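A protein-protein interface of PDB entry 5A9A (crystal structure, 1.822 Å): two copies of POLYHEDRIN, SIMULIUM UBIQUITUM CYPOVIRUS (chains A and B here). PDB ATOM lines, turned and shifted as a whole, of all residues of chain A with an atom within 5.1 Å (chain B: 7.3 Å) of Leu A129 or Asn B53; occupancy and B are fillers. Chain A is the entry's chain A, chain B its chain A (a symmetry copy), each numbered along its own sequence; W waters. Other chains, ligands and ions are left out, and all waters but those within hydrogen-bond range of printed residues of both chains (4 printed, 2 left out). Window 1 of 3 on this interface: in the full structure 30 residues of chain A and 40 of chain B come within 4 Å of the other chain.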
ATOM      1  N   GLU A 124      10.876  -2.196  31.680  1.00  0.00           N
ATOM      2  CA  GLU A 124      10.445  -2.785  30.419  1.00  0.00           C
ATOM      3  C   GLU A 124      10.247  -4.280  30.589  1.00  0.00           C
ATOM      4  O   GLU A 124      10.599  -4.839  31.628  1.00  0.00           O
ATOM      5  CB  GLU A 124      11.495  -2.519  29.340  1.00  0.00           C
ATOM      6  CG  GLU A 124      11.990  -1.077  29.299  1.00  0.00           C
ATOM      7  CD  GLU A 124      10.933  -0.107  28.799  1.00  0.00           C
ATOM      8  OE1 GLU A 124       9.782  -0.537  28.567  1.00  0.00           O
ATOM      9  OE2 GLU A 124      11.256   1.089  28.639  1.00  0.00           O
ATOM     10  N   ASN A 125       9.683  -4.930  29.575  1.00  0.00           N
ATOM     11  CA  ASN A 125       9.515  -6.377  29.618  1.00  0.00           C
ATOM     12  C   ASN A 125      10.803  -7.075  29.191  1.00  0.00           C
ATOM     13  O   ASN A 125      11.845  -6.434  29.056  1.00  0.00           O
ATOM     14  CB  ASN A 125       8.325  -6.824  28.760  1.00  0.00           C
ATOM     15  CG  ASN A 125       8.500  -6.503  27.290  1.00  0.00           C
ATOM     16  OD1 ASN A 125       9.619  -6.366  26.797  1.00  0.00           O
ATOM     17  ND2 ASN A 125       7.384  -6.387  26.578  1.00  0.00           N
ATOM     18  N   ASP A 127      11.928  -8.172  26.516  1.00  0.00           N
ATOM     19  CA  ASP A 127      12.533  -7.721  25.265  1.00  0.00           C
ATOM     20  C   ASP A 127      12.882  -6.234  25.335  1.00  0.00           C
ATOM     21  O   ASP A 127      13.208  -5.614  24.321  1.00  0.00           O
ATOM     22  CB  ASP A 127      11.591  -7.980  24.087  1.00  0.00           C
ATOM     23  CG  ASP A 127      11.443  -9.456  23.770  1.00  0.00           C
ATOM     24  OD1 ASP A 127      12.374 -10.232  24.074  1.00  0.00           O
ATOM     25  OD2 ASP A 127      10.398  -9.839  23.208  1.00  0.00           O
ATOM     26  N   CYS A 128      12.807  -5.676  26.538  1.00  0.00           N
ATOM     27  CA  CYS A 128      13.062  -4.256  26.764  1.00  0.00           C
ATOM     28  C   CYS A 128      12.149  -3.375  25.912  1.00  0.00           C
ATOM     29  O   CYS A 128      12.602  -2.409  25.296  1.00  0.00           O
ATOM     30  CB  CYS A 128      14.534  -3.923  26.499  1.00  0.00           C
ATOM     31  SG  CYS A 128      15.154  -2.537  27.497  1.00  0.00           S
ATOM     32  N   LEU A 129      10.863  -3.721  25.887  1.00  0.00           N
ATOM     33  CA  LEU A 129       9.845  -2.910  25.229  1.00  0.00           C
ATOM     34  C   LEU A 129       8.773  -2.551  26.257  1.00  0.00           C
ATOM     35  O   LEU A 129       8.612  -3.255  27.255  1.00  0.00           O
ATOM     36  CB  LEU A 129       9.213  -3.680  24.066  1.00  0.00           C
ATOM     37  CG  LEU A 129      10.133  -4.073  22.905  1.00  0.00           C
ATOM     38  CD1 LEU A 129       9.484  -5.152  22.050  1.00  0.00           C
ATOM     39  CD2 LEU A 129      10.497  -2.865  22.053  1.00  0.00           C
ATOM     40  N   ASN A 130       8.042  -1.463  26.023  1.00  0.00           N
ATOM     41  CA  ASN A 130       7.009  -1.036  26.962  1.00  0.00           C
ATOM     42  C   ASN A 130       5.598  -1.458  26.549  1.00  0.00           C
ATOM     43  O   ASN A 130       4.613  -1.051  27.168  1.00  0.00           O
ATOM     44  CB  ASN A 130       7.062   0.479  27.193  1.00  0.00           C
ATOM     45  CG  ASN A 130       7.066   1.272  25.902  1.00  0.00           C
ATOM     46  OD1 ASN A 130       6.425   0.896  24.922  1.00  0.00           O
ATOM     47  ND2 ASN A 130       7.798   2.378  25.896  1.00  0.00           N
ATOM     48  N   HIS A 131       5.500  -2.263  25.498  1.00  0.00           N
ATOM     49  CA  HIS A 131       4.246  -2.945  25.195  1.00  0.00           C
ATOM     50  C   HIS A 131       4.516  -4.397  24.820  1.00  0.00           C
ATOM     51  O   HIS A 131       5.607  -4.748  24.375  1.00  0.00           O
ATOM     52  CB  HIS A 131       3.467  -2.243  24.080  1.00  0.00           C
ATOM     53  CG  HIS A 131       2.006  -2.589  24.064  1.00  0.00           C
ATOM     54  ND1 HIS A 131       1.519  -3.736  23.482  1.00  0.00           N
ATOM     55  CD2 HIS A 131       0.931  -1.941  24.576  1.00  0.00           C
ATOM     56  CE1 HIS A 131       0.207  -3.782  23.629  1.00  0.00           C
ATOM     57  NE2 HIS A 131      -0.174  -2.707  24.291  1.00  0.00           N
ATOM     58  N   TRP A 134       5.605  -5.128  19.848  1.00  0.00           N
ATOM     59  CA  TRP A 134       6.475  -4.013  19.473  1.00  0.00           C
ATOM     60  C   TRP A 134       5.755  -2.998  18.591  1.00  0.00           C
ATOM     61  O   TRP A 134       6.123  -1.823  18.552  1.00  0.00           O
ATOM     62  CB  TRP A 134       7.735  -4.516  18.760  1.00  0.00           C
ATOM     63  CG  TRP A 134       7.500  -5.030  17.370  1.00  0.00           C
ATOM     64  CD1 TRP A 134       7.213  -6.314  17.006  1.00  0.00           C
ATOM     65  CD2 TRP A 134       7.543  -4.269  16.154  1.00  0.00           C
ATOM     66  NE1 TRP A 134       7.074  -6.401  15.641  1.00  0.00           N
ATOM     67  CE2 TRP A 134       7.263  -5.158  15.095  1.00  0.00           C
ATOM     68  CE3 TRP A 134       7.781  -2.922  15.860  1.00  0.00           C
ATOM     69  CZ2 TRP A 134       7.221  -4.745  13.763  1.00  0.00           C
ATOM     70  CZ3 TRP A 134       7.736  -2.512  14.537  1.00  0.00           C
ATOM     71  CH2 TRP A 134       7.460  -3.422  13.504  1.00  0.00           C
ATOM     72  N   ALA A 137       4.553  -0.431  20.749  1.00  0.00           N
ATOM     73  CA  ALA A 137       5.548   0.102  21.672  1.00  0.00           C
ATOM     74  C   ALA A 137       6.036   1.466  21.197  1.00  0.00           C
ATOM     75  O   ALA A 137       6.004   1.771  20.006  1.00  0.00           O
ATOM     76  CB  ALA A 137       6.711  -0.861  21.807  1.00  0.00           C
ATOM     77  N   LYS A 172      15.096   0.809  31.161  1.00  0.00           N
ATOM     78  CA  LYS A 172      15.529   1.860  30.243  1.00  0.00           C
ATOM     79  C   LYS A 172      15.341   3.202  30.940  1.00  0.00           C
ATOM     80  O   LYS A 172      14.336   3.411  31.619  1.00  0.00           O
ATOM     81  CB  LYS A 172      14.721   1.812  28.940  1.00  0.00           C
ATOM     82  CG  LYS A 172      15.340   2.608  27.792  1.00  0.00           C
ATOM     83  CD  LYS A 172      14.622   2.355  26.463  1.00  0.00           C
ATOM     84  CE  LYS A 172      13.275   3.065  26.402  1.00  0.00           C
ATOM     85  NZ  LYS A 172      12.603   2.895  25.076  1.00  0.00           N
ATOM     86  N   ILE B  33       8.339   2.410  18.160  1.00  0.00           N
ATOM     87  CA  ILE B  33       9.540   1.586  18.161  1.00  0.00           C
ATOM     88  C   ILE B  33       9.789   0.936  16.803  1.00  0.00           C
ATOM     89  O   ILE B  33       8.857   0.523  16.116  1.00  0.00           O
ATOM     90  CB  ILE B  33       9.454   0.481  19.237  1.00  0.00           C
ATOM     91  CG1 ILE B  33       9.664   1.079  20.632  1.00  0.00           C
ATOM     92  CG2 ILE B  33      10.479  -0.613  18.971  1.00  0.00           C
ATOM     93  CD1 ILE B  33      11.048   1.657  20.851  1.00  0.00           C
ATOM     94  N   LYS B  34      11.062   0.861  16.427  1.00  0.00           N
ATOM     95  CA  LYS B  34      11.491   0.066  15.281  1.00  0.00           C
ATOM     96  C   LYS B  34      12.237  -1.139  15.828  1.00  0.00           C
ATOM     97  O   LYS B  34      12.874  -1.042  16.876  1.00  0.00           O
ATOM     98  CB  LYS B  34      12.405   0.877  14.357  1.00  0.00           C
ATOM     99  CG  LYS B  34      11.690   1.960  13.550  1.00  0.00           C
ATOM    100  CD  LYS B  34      11.313   3.148  14.421  1.00  0.00           C
ATOM    101  CE  LYS B  34      10.414   4.125  13.680  1.00  0.00           C
ATOM    102  NZ  LYS B  34       9.892   5.177  14.593  1.00  0.00           N
ATOM    103  N   ARG B  35      12.163  -2.270  15.131  1.00  0.00           N
ATOM    104  CA  ARG B  35      12.757  -3.502  15.639  1.00  0.00           C
ATOM    105  C   ARG B  35      13.521  -4.268  14.559  1.00  0.00           C
ATOM    106  O   ARG B  35      12.993  -4.558  13.484  1.00  0.00           O
ATOM    107  CB  ARG B  35      11.678  -4.387  16.271  1.00  0.00           C
ATOM    108  CG  ARG B  35      12.228  -5.525  17.121  1.00  0.00           C
ATOM    109  CD  ARG B  35      11.176  -6.069  18.079  1.00  0.00           C
ATOM    110  NE  ARG B  35      11.731  -7.070  18.988  1.00  0.00           N
ATOM    111  CZ  ARG B  35      11.005  -7.843  19.792  1.00  0.00           C
ATOM    112  NH1 ARG B  35       9.681  -7.746  19.801  1.00  0.00           N
ATOM    113  NH2 ARG B  35      11.603  -8.723  20.584  1.00  0.00           N
ATOM    114  N   VAL B  36      14.776  -4.583  14.861  1.00  0.00           N
ATOM    115  CA  VAL B  36      15.652  -5.275  13.926  1.00  0.00           C
ATOM    116  C   VAL B  36      16.233  -6.524  14.576  1.00  0.00           C
ATOM    117  O   VAL B  36      16.734  -6.476  15.703  1.00  0.00           O
ATOM    118  CB  VAL B  36      16.824  -4.368  13.486  1.00  0.00           C
ATOM    119  CG1 VAL B  36      17.913  -5.184  12.796  1.00  0.00           C
ATOM    120  CG2 VAL B  36      16.327  -3.256  12.579  1.00  0.00           C
ATOM    121  N   ASP B  51      18.532  -9.044  19.074  1.00  0.00           N
ATOM    122  CA  ASP B  51      17.309  -8.268  18.920  1.00  0.00           C
ATOM    123  C   ASP B  51      17.525  -6.808  19.315  1.00  0.00           C
ATOM    124  O   ASP B  51      17.890  -6.512  20.453  1.00  0.00           O
ATOM    125  CB  ASP B  51      16.208  -8.904  19.774  1.00  0.00           C
ATOM    126  CG  ASP B  51      14.944  -8.068  19.828  1.00  0.00           C
ATOM    127  OD1 ASP B  51      14.653  -7.360  18.845  1.00  0.00           O
ATOM    128  OD2 ASP B  51      14.237  -8.122  20.858  1.00  0.00           O
ATOM    129  N   TYR B  52      17.294  -5.902  18.367  1.00  0.00           N
ATOM    130  CA  TYR B  52      17.474  -4.470  18.592  1.00  0.00           C
ATOM    131  C   TYR B  52      16.137  -3.741  18.552  1.00  0.00           C
ATOM    132  O   TYR B  52      15.242  -4.114  17.791  1.00  0.00           O
ATOM    133  CB  TYR B  52      18.360  -3.851  17.506  1.00  0.00           C
ATOM    134  CG  TYR B  52      19.826  -4.230  17.534  1.00  0.00           C
ATOM    135  CD1 TYR B  52      20.279  -5.381  16.907  1.00  0.00           C
ATOM    136  CD2 TYR B  52      20.763  -3.407  18.148  1.00  0.00           C
ATOM    137  CE1 TYR B  52      21.622  -5.722  16.917  1.00  0.00           C
ATOM    138  CE2 TYR B  52      22.105  -3.737  18.162  1.00  0.00           C
ATOM    139  CZ  TYR B  52      22.529  -4.895  17.544  1.00  0.00           C
ATOM    140  OH  TYR B  52      23.864  -5.223  17.553  1.00  0.00           O
ATOM    141  N   ASN B  53      16.005  -2.694  19.359  1.00  0.00           N
ATOM    142  CA  ASN B  53      14.878  -1.777  19.215  1.00  0.00           C
ATOM    143  C   ASN B  53      15.271  -0.340  19.550  1.00  0.00           C
ATOM    144  O   ASN B  53      16.142  -0.098  20.389  1.00  0.00           O
ATOM    145  CB  ASN B  53      13.671  -2.231  20.052  1.00  0.00           C
ATOM    146  CG  ASN B  53      13.756  -1.793  21.508  1.00  0.00           C
ATOM    147  OD1 ASN B  53      13.702  -0.602  21.817  1.00  0.00           O
ATOM    148  ND2 ASN B  53      13.859  -2.758  22.409  1.00  0.00           N
ATOM    149  N   ALA B  54      14.638   0.610  18.869  1.00  0.00           N
ATOM    150  CA  ALA B  54      14.873   2.029  19.116  1.00  0.00           C
ATOM    151  C   ALA B  54      13.772   2.848  18.449  1.00  0.00           C
ATOM    152  O   ALA B  54      13.149   2.393  17.490  1.00  0.00           O
ATOM    153  CB  ALA B  54      16.233   2.447  18.594  1.00  0.00           C
ATOM    154  N   PRO B  55      13.511   4.053  18.972  1.00  0.00           N
ATOM    155  CA  PRO B  55      12.438   4.891  18.428  1.00  0.00           C
ATOM    156  C   PRO B  55      12.879   5.873  17.339  1.00  0.00           C
ATOM    157  O   PRO B  55      12.016   6.358  16.605  1.00  0.00           O
ATOM    158  CB  PRO B  55      11.941   5.647  19.660  1.00  0.00           C
ATOM    159  CG  PRO B  55      13.154   5.792  20.513  1.00  0.00           C
ATOM    160  CD  PRO B  55      14.027   4.582  20.247  1.00  0.00           C
ATOM    161  N   GLU B  56      14.174   6.166  17.227  1.00  0.00           N
ATOM    162  CA  GLU B  56      14.645   7.098  16.200  1.00  0.00           C
ATOM    163  C   GLU B  56      15.429   6.384  15.094  1.00  0.00           C
ATOM    164  O   GLU B  56      15.110   6.513  13.914  1.00  0.00           O
ATOM    165  CB  GLU B  56      15.502   8.209  16.813  1.00  0.00           C
ATOM    166  CG  GLU B  56      14.977   8.759  18.129  1.00  0.00           C
ATOM    167  CD  GLU B  56      13.522   9.183  18.054  1.00  0.00           C
ATOM    168  OE1 GLU B  56      13.040   9.504  16.945  1.00  0.00           O
ATOM    169  OE2 GLU B  56      12.857   9.192  19.110  1.00  0.00           O
ATOM    170  N   PHE B  57      16.461   5.641  15.475  1.00  0.00           N
ATOM    171  CA  PHE B  57      17.228   4.860  14.506  1.00  0.00           C
ATOM    172  C   PHE B  57      18.011   3.743  15.177  1.00  0.00           C
ATOM    173  O   PHE B  57      18.527   3.912  16.279  1.00  0.00           O
ATOM    174  CB  PHE B  57      18.182   5.756  13.700  1.00  0.00           C
ATOM    175  CG  PHE B  57      19.154   6.529  14.541  1.00  0.00           C
ATOM    176  CD1 PHE B  57      20.384   5.987  14.881  1.00  0.00           C
ATOM    177  CD2 PHE B  57      18.849   7.808  14.976  1.00  0.00           C
ATOM    178  CE1 PHE B  57      21.285   6.703  15.655  1.00  0.00           C
ATOM    179  CE2 PHE B  57      19.744   8.530  15.745  1.00  0.00           C
ATOM    180  CZ  PHE B  57      20.963   7.977  16.086  1.00  0.00           C
ATOM    181  N   ILE B  58      18.084   2.597  14.504  1.00  0.00           N
ATOM    182  CA  ILE B  58      18.912   1.492  14.965  1.00  0.00           C
ATOM    183  C   ILE B  58      20.173   1.409  14.126  1.00  0.00           C
ATOM    184  O   ILE B  58      20.141   0.944  12.987  1.00  0.00           O
ATOM    185  CB  ILE B  58      18.190   0.137  14.856  1.00  0.00           C
ATOM    186  CG1 ILE B  58      16.945   0.115  15.743  1.00  0.00           C
ATOM    187  CG2 ILE B  58      19.135  -0.992  15.255  1.00  0.00           C
ATOM    188  CD1 ILE B  58      16.062  -1.093  15.512  1.00  0.00           C
ATOM    189  N   ASN B 198      16.766   8.197  21.672  1.00  0.00           N
ATOM    190  CA  ASN B 198      17.312   7.084  20.910  1.00  0.00           C
ATOM    191  C   ASN B 198      18.293   6.264  21.736  1.00  0.00           C
ATOM    192  O   ASN B 198      19.509   6.376  21.591  1.00  0.00           O
ATOM    193  CB  ASN B 198      17.946   7.545  19.597  1.00  0.00           C
ATOM    194  CG  ASN B 198      17.942   6.452  18.549  1.00  0.00           C
ATOM    195  OD1 ASN B 198      16.880   5.942  18.182  1.00  0.00           O
ATOM    196  ND2 ASN B 198      19.125   6.074  18.066  1.00  0.00           N
ATOM    197  N   ILE B 199      17.727   5.449  22.617  1.00  0.00           N
ATOM    198  CA  ILE B 199      18.478   4.465  23.373  1.00  0.00           C
ATOM    199  C   ILE B 199      18.375   3.147  22.617  1.00  0.00           C
ATOM    200  O   ILE B 199      17.358   2.455  22.689  1.00  0.00           O
ATOM    201  CB  ILE B 199      17.900   4.307  24.786  1.00  0.00           C
ATOM    202  CG1 ILE B 199      17.812   5.673  25.469  1.00  0.00           C
ATOM    203  CG2 ILE B 199      18.747   3.350  25.608  1.00  0.00           C
ATOM    204  CD1 ILE B 199      16.969   5.681  26.723  1.00  0.00           C
ATOM    205  N   ILE B 200      19.424   2.820  21.873  1.00  0.00           N
ATOM    206  CA  ILE B 200      19.419   1.643  21.017  1.00  0.00           C
ATOM    207  C   ILE B 200      19.639   0.391  21.862  1.00  0.00           C
ATOM    208  O   ILE B 200      20.744   0.135  22.339  1.00  0.00           O
ATOM    209  CB  ILE B 200      20.505   1.747  19.929  1.00  0.00           C
ATOM    210  CG1 ILE B 200      20.338   3.056  19.150  1.00  0.00           C
ATOM    211  CG2 ILE B 200      20.433   0.559  18.983  1.00  0.00           C
ATOM    212  CD1 ILE B 200      21.531   3.416  18.290  1.00  0.00           C
ATOM    213  N   ILE B 201      18.572  -0.376  22.057  1.00  0.00           N
ATOM    214  CA  ILE B 201      18.649  -1.587  22.860  1.00  0.00           C
ATOM    215  C   ILE B 201      19.295  -2.718  22.074  1.00  0.00           C
ATOM    216  O   ILE B 201      18.828  -3.084  20.997  1.00  0.00           O
ATOM    217  CB  ILE B 201      17.253  -2.065  23.317  1.00  0.00           C
ATOM    218  CG1 ILE B 201      16.482  -0.932  24.001  1.00  0.00           C
ATOM    219  CG2 ILE B 201      17.383  -3.262  24.256  1.00  0.00           C
ATOM    220  CD1 ILE B 201      17.148  -0.403  25.253  1.00  0.00           C
ATOM    221  N   ARG B 202      20.378  -3.262  22.615  1.00  0.00           N
ATOM    222  CA  ARG B 202      20.962  -4.491  22.097  1.00  0.00           C
ATOM    223  C   ARG B 202      20.696  -5.591  23.108  1.00  0.00           C
ATOM    224  O   ARG B 202      21.413  -5.714  24.103  1.00  0.00           O
ATOM    225  CB  ARG B 202      22.469  -4.328  21.884  1.00  0.00           C
ATOM    226  CG  ARG B 202      23.143  -5.489  21.149  1.00  0.00           C
ATOM    227  CD  ARG B 202      24.660  -5.311  21.157  1.00  0.00           C
ATOM    228  NE  ARG B 202      25.372  -6.268  20.313  1.00  0.00           N
ATOM    229  CZ  ARG B 202      25.839  -7.444  20.728  1.00  0.00           C
ATOM    230  NH1 ARG B 202      25.668  -7.833  21.985  1.00  0.00           N
ATOM    231  NH2 ARG B 202      26.488  -8.233  19.884  1.00  0.00           N
ATOM    232  N   ASN B 203      19.646  -6.372  22.871  1.00  0.00           N
ATOM    233  CA  ASN B 203      19.314  -7.481  23.754  1.00  0.00           C
ATOM    234  C   ASN B 203      20.385  -8.559  23.656  1.00  0.00           C
ATOM    235  O   ASN B 203      21.055  -8.687  22.629  1.00  0.00           O
ATOM    236  CB  ASN B 203      17.940  -8.059  23.403  1.00  0.00           C
ATOM    237  CG  ASN B 203      16.799  -7.119  23.765  1.00  0.00           C
ATOM    238  OD1 ASN B 203      15.984  -6.754  22.916  1.00  0.00           O
ATOM    239  ND2 ASN B 203      16.739  -6.723  25.030  1.00  0.00           N
ATOM    240  N   LYS B 221       7.270 -12.824  17.767  1.00  0.00           N
ATOM    241  CA  LYS B 221       7.647 -11.423  17.932  1.00  0.00           C
ATOM    242  C   LYS B 221       7.145 -10.572  16.767  1.00  0.00           C
ATOM    243  O   LYS B 221       7.321  -9.354  16.757  1.00  0.00           O
ATOM    244  CB  LYS B 221       9.166 -11.288  18.038  1.00  0.00           C
ATOM    245  CG  LYS B 221       9.810 -12.181  19.092  1.00  0.00           C
ATOM    246  CD  LYS B 221       9.301 -11.888  20.496  1.00  0.00           C
ATOM    247  CE  LYS B 221       9.937 -12.837  21.504  1.00  0.00           C
ATOM    248  NZ  LYS B 221       9.492 -12.594  22.902  1.00  0.00           N
HETATM  249  O   HOH W   1      14.549   1.927  22.612  1.00  0.00           O
HETATM  250  O   HOH W   2       8.347  -8.706  22.150  1.00  0.00           O
HETATM  251  O   HOH W   3      12.163   0.048  24.201  1.00  0.00           O
HETATM  252  O   HOH W   4       6.469  -8.002  20.059  1.00  0.00           O
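Water W2 lies within hydrogen-bond range of OD2 of Asp A127 (2.6 Å) and NH1 of Arg B35 (2.9 Å). Water W3 lies within hydrogen-bond range of O of Cys A128, OD1 of Asn B53 and NZ of Lys A172. Water W1 lies within hydrogen-bond range of OD1 of Asn B53 (2.8 Å), O of Ile B199 (2.9 Å) and NZ of Lys A172 (3.3 Å). Water W4 lies within hydrogen-bond range of N of Trp A134 (3.0 Å) and NH1 of Arg B35 (3.2 Å).
No position is printed for both chains. Of the 16 pairs that touch across the chains among the printed residues, none has its exchanged pair printed and touching as well.
The backbone carbonyl oxygen (O) of Cys A128 is in hydrogen-bond range of the side-chain amide nitrogen (ND2) of Asn B53. O of Asp A127 sits at hydrogen-bond distance from ND2 of Asn B53, at 3.5 Å. The backbone NH of Ile B33 lies within hydrogen-bond range of the backbone carbonyl oxygen of Ala A137 (3.0 Å). The side-chain amide oxygen of Asn B203 lies close to the backbone carbonyl oxygen of Asp A127 (3.3 Å). OD2 of Asp A127 is in salt-bridge range of NH2 of Arg B35 (3.1 Å). The side-chain carboxylate (OD2) of Asp A127 lies within salt-bridge range of the side-chain amino group (NZ) of Lys B221. O of Lys B221 sits close to NE1 of Trp A134, 3.2 Å away.
The side-chain amide oxygen (OD1) of Asn A125 lies within hydrogen-bond range of the backbone NH (N) of Leu A129, 3.1 Å away. The backbone NH (N) of Asp A127 lies within hydrogen-bond range of the side-chain amide oxygen (OD1) of Asn A125 (2.9 Å). The backbone NH (N) of Ile B201 is in hydrogen-bond range of the backbone carbonyl oxygen (O) of Asn B53. The side-chain carboxylate of Asp B51 lies within salt-bridge range of the guanidinium group of Arg B35 (2.7 Å). The backbone NH (N) of Asn B203 lies within hydrogen-bond range of the backbone carbonyl oxygen (O) of Asp B51 (3.0 Å). OD1 of Asn A125 lies within hydrogen-bond range of N of Cys A128 (3.3 Å).
Cys A128 touches Ile B201. Cys A128 touches Asn B203. Ile B33 touches Leu A129 (CG2 to CD2, 3.8 Å). Leu A129 touches Arg B35. Leu A129 touches Asn B53. O of Ile B33 touches CZ3 of Trp A134 (3.6 Å). Arg B35 touches Trp A134. CG of Lys A172 touches CD1 of Ile B199, at 3.6 Å. Ile B201 touches Lys A172 (CD1 to CD, 3.9 Å).
Of the 19 printed residues of chain B, 7 touch a printed residue of chain A. Hydrophobic or aromatic side chains of chain A that line the printed part of chain B: Leu A129, Trp A134 and Ala A137. Among the printed residues, Asp or Glu carboxylates within 4 Å of a Lys or Arg side-chain nitrogen of the other chain: Asp A127 with Arg B35 (3.1 Å) and Asp A127 with Lys B221 (2.9 Å).
Leu A129 touches just these residues of chain B: Ile B33, Arg B35 and Asn B53. Printed residues of chain B within 4 Å of Ala A137: Ile B33. Asn B53 touches just these residues of chain A: Asp A127, Cys A128 and Leu A129. Asn B198 touches none of the printed residues of chain A. Of the printed residues of chain A, Ile B199 touches Lys A172. Of the printed residues of chain A, Ile B201 touches Cys A128 (3.7 Å) and Lys A172 (3.9 Å). Of the printed residues of chain A, Asn B203 touches Asp A127 and Cys A128. The nearest printed residue of chain B that does not touch Lys A172 is Ile B33 (4.7 Å).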
